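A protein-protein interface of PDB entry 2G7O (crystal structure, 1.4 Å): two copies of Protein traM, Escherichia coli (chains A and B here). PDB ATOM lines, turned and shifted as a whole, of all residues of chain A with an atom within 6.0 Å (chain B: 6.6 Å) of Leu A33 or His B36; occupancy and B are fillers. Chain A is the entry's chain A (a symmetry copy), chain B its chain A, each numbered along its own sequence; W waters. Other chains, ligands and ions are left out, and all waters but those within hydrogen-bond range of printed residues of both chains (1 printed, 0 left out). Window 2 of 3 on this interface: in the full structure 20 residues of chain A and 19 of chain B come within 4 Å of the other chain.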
ATOM      1  N   LEU A  28     -24.233  -4.491 -15.697  1.00  0.00           N
ATOM      2  CA  LEU A  28     -23.417  -5.439 -14.947  1.00  0.00           C
ATOM      3  C   LEU A  28     -22.695  -6.363 -15.914  1.00  0.00           C
ATOM      4  O   LEU A  28     -21.503  -6.640 -15.749  1.00  0.00           O
ATOM      5  CB  LEU A  28     -24.291  -6.240 -13.972  1.00  0.00           C
ATOM      6  CG  LEU A  28     -23.517  -7.210 -13.070  1.00  0.00           C
ATOM      7  CD1 LEU A  28     -22.663  -6.484 -12.038  1.00  0.00           C
ATOM      8  CD2 LEU A  28     -24.471  -8.182 -12.356  1.00  0.00           C
ATOM      9  N   GLY A  29     -23.399  -6.859 -16.924  1.00  0.00           N
ATOM     10  CA  GLY A  29     -22.761  -7.738 -17.902  1.00  0.00           C
ATOM     11  C   GLY A  29     -21.669  -7.007 -18.661  1.00  0.00           C
ATOM     12  O   GLY A  29     -20.576  -7.561 -18.875  1.00  0.00           O
ATOM     13  N   ILE A  30     -21.944  -5.780 -19.108  1.00  0.00           N
ATOM     14  CA  ILE A  30     -20.913  -5.022 -19.838  1.00  0.00           C
ATOM     15  C   ILE A  30     -19.688  -4.773 -18.950  1.00  0.00           C
ATOM     16  O   ILE A  30     -18.542  -4.940 -19.395  1.00  0.00           O
ATOM     17  CB  ILE A  30     -21.487  -3.699 -20.370  1.00  0.00           C
ATOM     18  CG1 ILE A  30     -22.554  -3.986 -21.448  1.00  0.00           C
ATOM     19  CG2 ILE A  30     -20.354  -2.809 -20.930  1.00  0.00           C
ATOM     20  CD1 ILE A  30     -23.408  -2.753 -21.833  1.00  0.00           C
ATOM     21  N   GLU A  31     -19.918  -4.390 -17.700  1.00  0.00           N
ATOM     22  CA  GLU A  31     -18.819  -4.103 -16.780  1.00  0.00           C
ATOM     23  C   GLU A  31     -17.980  -5.343 -16.477  1.00  0.00           C
ATOM     24  O   GLU A  31     -16.760  -5.253 -16.281  1.00  0.00           O
ATOM     25  CB  GLU A  31     -19.337  -3.489 -15.473  1.00  0.00           C
ATOM     26  CG  GLU A  31     -19.825  -2.062 -15.616  1.00  0.00           C
ATOM     27  CD  GLU A  31     -18.688  -1.074 -15.674  1.00  0.00           C
ATOM     28  OE1 GLU A  31     -17.546  -1.422 -16.040  1.00  0.00           O
ATOM     29  OE2 GLU A  31     -18.958   0.087 -15.327  1.00  0.00           O
ATOM     30  N   SER A  32     -18.625  -6.504 -16.433  1.00  0.00           N
ATOM     31  CA  SER A  32     -17.885  -7.761 -16.212  1.00  0.00           C
ATOM     32  C   SER A  32     -16.858  -8.039 -17.323  1.00  0.00           C
ATOM     33  O   SER A  32     -15.865  -8.751 -17.088  1.00  0.00           O
ATOM     34  CB  SER A  32     -18.856  -8.944 -16.079  1.00  0.00           C
ATOM     35  OG  SER A  32     -19.295  -9.420 -17.346  1.00  0.00           O
ATOM     36  N   LEU A  33     -17.085  -7.471 -18.509  1.00  0.00           N
ATOM     37  CA  LEU A  33     -16.230  -7.681 -19.671  1.00  0.00           C
ATOM     38  C   LEU A  33     -15.121  -6.640 -19.737  1.00  0.00           C
ATOM     39  O   LEU A  33     -14.268  -6.705 -20.647  1.00  0.00           O
ATOM     40  CB  LEU A  33     -17.085  -7.650 -20.961  1.00  0.00           C
ATOM     41  CG  LEU A  33     -17.975  -8.871 -21.251  1.00  0.00           C
ATOM     42  CD1 LEU A  33     -19.018  -8.587 -22.337  1.00  0.00           C
ATOM     43  CD2 LEU A  33     -17.134 -10.076 -21.659  1.00  0.00           C
ATOM     44  N   SER A  34     -15.103  -5.695 -18.792  1.00  0.00           N
ATOM     45  CA  SER A  34     -14.106  -4.632 -18.808  1.00  0.00           C
ATOM     46  C   SER A  34     -12.699  -5.204 -18.608  1.00  0.00           C
ATOM     47  O   SER A  34     -12.482  -6.019 -17.710  1.00  0.00           O
ATOM     48  CB  SER A  34     -14.325  -3.602 -17.699  1.00  0.00           C
ATOM     49  OG  SER A  34     -13.559  -2.464 -18.022  1.00  0.00           O
ATOM     50  N   PRO A  35     -11.721  -4.728 -19.405  1.00  0.00           N
ATOM     51  CA  PRO A  35     -10.370  -5.287 -19.250  1.00  0.00           C
ATOM     52  C   PRO A  35      -9.724  -5.081 -17.873  1.00  0.00           C
ATOM     53  O   PRO A  35      -8.925  -5.913 -17.454  1.00  0.00           O
ATOM     54  CB  PRO A  35      -9.547  -4.578 -20.341  1.00  0.00           C
ATOM     55  CG  PRO A  35     -10.398  -3.512 -20.920  1.00  0.00           C
ATOM     56  CD  PRO A  35     -11.812  -3.700 -20.458  1.00  0.00           C
ATOM     57  N   VAL A  37     -10.947  -5.519 -14.964  1.00  0.00           N
ATOM     58  CA  VAL A  37     -11.318  -6.564 -14.004  1.00  0.00           C
ATOM     59  C   VAL A  37     -11.119  -8.011 -14.500  1.00  0.00           C
ATOM     60  O   VAL A  37     -11.467  -8.961 -13.818  1.00  0.00           O
ATOM     61  CB  VAL A  37     -12.705  -6.322 -13.344  1.00  0.00           C
ATOM     62  CG1 VAL A  37     -12.656  -5.062 -12.441  1.00  0.00           C
ATOM     63  CG2 VAL A  37     -13.805  -6.198 -14.379  1.00  0.00           C
ATOM     64  N   GLU B  31     -22.309   3.031 -21.651  1.00  0.00           N
ATOM     65  CA  GLU B  31     -21.744   1.682 -21.655  1.00  0.00           C
ATOM     66  C   GLU B  31     -21.891   0.998 -23.012  1.00  0.00           C
ATOM     67  O   GLU B  31     -21.027   0.214 -23.425  1.00  0.00           O
ATOM     68  CB  GLU B  31     -22.377   0.815 -20.559  1.00  0.00           C
ATOM     69  CG  GLU B  31     -21.942   1.184 -19.155  1.00  0.00           C
ATOM     70  CD  GLU B  31     -20.567   0.661 -18.829  1.00  0.00           C
ATOM     71  OE1 GLU B  31     -19.741   0.401 -19.729  1.00  0.00           O
ATOM     72  OE2 GLU B  31     -20.319   0.498 -17.623  1.00  0.00           O
ATOM     73  N   LEU B  33     -21.446   2.302 -25.761  1.00  0.00           N
ATOM     74  CA  LEU B  33     -20.418   2.875 -26.622  1.00  0.00           C
ATOM     75  C   LEU B  33     -19.033   2.373 -26.239  1.00  0.00           C
ATOM     76  O   LEU B  33     -18.042   2.729 -26.911  1.00  0.00           O
ATOM     77  CB  LEU B  33     -20.478   4.420 -26.550  1.00  0.00           C
ATOM     78  CG  LEU B  33     -21.641   5.119 -27.277  1.00  0.00           C
ATOM     79  CD1 LEU B  33     -21.798   6.583 -26.852  1.00  0.00           C
ATOM     80  CD2 LEU B  33     -21.462   5.048 -28.790  1.00  0.00           C
ATOM     81  N   SER B  34     -18.942   1.548 -25.192  1.00  0.00           N
ATOM     82  CA  SER B  34     -17.650   1.059 -24.728  1.00  0.00           C
ATOM     83  C   SER B  34     -16.988   0.178 -25.792  1.00  0.00           C
ATOM     84  O   SER B  34     -17.635  -0.707 -26.354  1.00  0.00           O
ATOM     85  CB  SER B  34     -17.761   0.211 -23.460  1.00  0.00           C
ATOM     86  OG  SER B  34     -16.468   0.105 -22.908  1.00  0.00           O
ATOM     87  N   PRO B  35     -15.675   0.373 -26.025  1.00  0.00           N
ATOM     88  CA  PRO B  35     -15.028  -0.441 -27.064  1.00  0.00           C
ATOM     89  C   PRO B  35     -15.039  -1.956 -26.818  1.00  0.00           C
ATOM     90  O   PRO B  35     -15.057  -2.721 -27.778  1.00  0.00           O
ATOM     91  CB  PRO B  35     -13.583   0.086 -27.106  1.00  0.00           C
ATOM     92  CG  PRO B  35     -13.415   1.015 -25.963  1.00  0.00           C
ATOM     93  CD  PRO B  35     -14.758   1.329 -25.376  1.00  0.00           C
ATOM     94  N   HIS B  36     -15.072  -2.413 -25.566  1.00  0.00           N
ATOM     95  CA  HIS B  36     -15.044  -3.872 -25.344  1.00  0.00           C
ATOM     96  C   HIS B  36     -16.350  -4.606 -25.670  1.00  0.00           C
ATOM     97  O   HIS B  36     -16.372  -5.842 -25.750  1.00  0.00           O
ATOM     98  CB  HIS B  36     -14.529  -4.242 -23.950  1.00  0.00           C
ATOM     99  CG  HIS B  36     -15.384  -3.730 -22.834  1.00  0.00           C
ATOM    100  ND1 HIS B  36     -15.338  -2.426 -22.404  1.00  0.00           N
ATOM    101  CD2 HIS B  36     -16.290  -4.358 -22.047  1.00  0.00           C
ATOM    102  CE1 HIS B  36     -16.191  -2.267 -21.405  1.00  0.00           C
ATOM    103  NE2 HIS B  36     -16.785  -3.424 -21.177  1.00  0.00           N
ATOM    104  N   VAL B  37     -17.427  -3.853 -25.896  1.00  0.00           N
ATOM    105  CA  VAL B  37     -18.655  -4.495 -26.378  1.00  0.00           C
ATOM    106  C   VAL B  37     -19.037  -4.168 -27.836  1.00  0.00           C
ATOM    107  O   VAL B  37     -20.078  -4.581 -28.319  1.00  0.00           O
ATOM    108  CB  VAL B  37     -19.842  -4.366 -25.383  1.00  0.00           C
ATOM    109  CG1 VAL B  37     -19.548  -5.171 -24.091  1.00  0.00           C
ATOM    110  CG2 VAL B  37     -20.146  -2.918 -25.057  1.00  0.00           C
ATOM    111  N   SER B  38     -18.160  -3.463 -28.554  1.00  0.00           N
ATOM    112  CA  SER B  38     -18.372  -3.275 -30.004  1.00  0.00           C
ATOM    113  C   SER B  38     -18.485  -4.639 -30.689  1.00  0.00           C
ATOM    114  O   SER B  38     -17.720  -5.567 -30.382  1.00  0.00           O
ATOM    115  CB  SER B  38     -17.263  -2.432 -30.645  1.00  0.00           C
ATOM    116  OG  SER B  38     -16.036  -3.148 -30.719  1.00  0.00           O
ATOM    117  N   ASN B  40     -20.710  -6.853 -30.244  1.00  0.00           N
ATOM    118  CA  ASN B  40     -21.427  -7.810 -29.425  1.00  0.00           C
ATOM    119  C   ASN B  40     -22.917  -7.475 -29.504  1.00  0.00           C
ATOM    120  O   ASN B  40     -23.384  -6.491 -28.914  1.00  0.00           O
ATOM    121  CB  ASN B  40     -20.919  -7.759 -27.982  1.00  0.00           C
ATOM    122  CG  ASN B  40     -21.489  -8.869 -27.121  1.00  0.00           C
ATOM    123  OD1 ASN B  40     -22.618  -9.330 -27.337  1.00  0.00           O
ATOM    124  ND2 ASN B  40     -20.719  -9.295 -26.119  1.00  0.00           N
ATOM    125  N   PHE B  43     -25.253  -6.404 -26.574  1.00  0.00           N
ATOM    126  CA  PHE B  43     -25.113  -5.086 -25.956  1.00  0.00           C
ATOM    127  C   PHE B  43     -25.226  -3.911 -26.936  1.00  0.00           C
ATOM    128  O   PHE B  43     -24.941  -2.757 -26.583  1.00  0.00           O
ATOM    129  CB  PHE B  43     -23.829  -5.044 -25.139  1.00  0.00           C
ATOM    130  CG  PHE B  43     -23.783  -6.082 -24.042  1.00  0.00           C
ATOM    131  CD1 PHE B  43     -24.740  -6.094 -23.023  1.00  0.00           C
ATOM    132  CD2 PHE B  43     -22.776  -7.052 -24.023  1.00  0.00           C
ATOM    133  CE1 PHE B  43     -24.684  -7.049 -22.025  1.00  0.00           C
ATOM    134  CE2 PHE B  43     -22.716  -7.999 -23.040  1.00  0.00           C
ATOM    135  CZ  PHE B  43     -23.671  -8.002 -22.026  1.00  0.00           C
HETATM  136  O   HOH W   1     -17.450  -1.054 -19.030  1.00  0.00           O
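Water W1 lies within hydrogen-bond range of OE1 of Glu B31, OE1 of Glu A31 and NE2 of His B36.
OG of Ser B34 lies within hydrogen-bond range of ND1 of His B36, 2.8 Å away.
Printed residues of chain A that touch a printed residue of chain B: Ile A30, Glu A31, Leu A33 and Ser A34.
Along chain A the printed residues that touch a printed residue of chain B span positions 30 to 34.
Of the 9 printed residues of chain B, 4 touch a printed residue of chain A.
Printed residues of chain B that touch a printed residue of chain A: Glu B31, His B36, Val B37 and Phe B43.
Hydrophobic or aromatic side chains of chain B that line the printed part of chain A: His B36, Val B37 and Phe B43.
Among the printed residues, 8 pairs touch across the chains.
Among the printed residues, no Asp or Glu carboxylate lies within 4 Å of a Lys or Arg side-chain nitrogen of the other chain.
Among the printed residues, merely in contact across the chains: Leu A33 with His B36, Ile A30 with Phe B43, Ile A30 with Glu B31, Ser A34 with His B36, Leu A33 with Phe B43 and Leu A33 with Val B37.
OE2 of Glu B31 lies close to OE2 of Glu A31, at 2.7 Å.
The backbone carbonyl oxygen of Ile A30 sits at hydrogen-bond distance from a ring nitrogen (NE2) of His B36 (2.9 Å).
Glu B31 touches its own counterpart, Glu A31.
Leu A33 touches Val B37, but with the chains exchanged Val A37 does not touch Leu B33 (15.5 Å).
Of the 8 pairs that touch across the chains among the printed residues, 1 has its exchanged pair printed and touching as well.
Leu A33 touches three residues of chain B.
Of the printed residues of chain A, His B36 touches Ile A30 (2.9 Å), Leu A33 (3.4 Å) and Ser A34 (3.7 Å).
Printed residues of chain B within 4 Å of Ile A30: Glu B31, His B36 and Phe B43.
Printed residues of chain B within 4 Å of Ser A34: His B36.
Of the printed residues of chain A, Glu B31 touches Ile A30 and Glu A31.
Printed residues of chain A within 4 Å of Val B37: Leu A33 (3.9 Å).
Printed residues of chain A within 4 Å of Phe B43: Ile A30 (3.4 Å) and Leu A33 (3.8 Å).
Ser B38 touches none of the printed residues of chain A.
Pro A35 touches none of the printed residues of chain B.
The nearest printed residue of chain A that does not touch His B36 is Pro A35 (4.2 Å).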
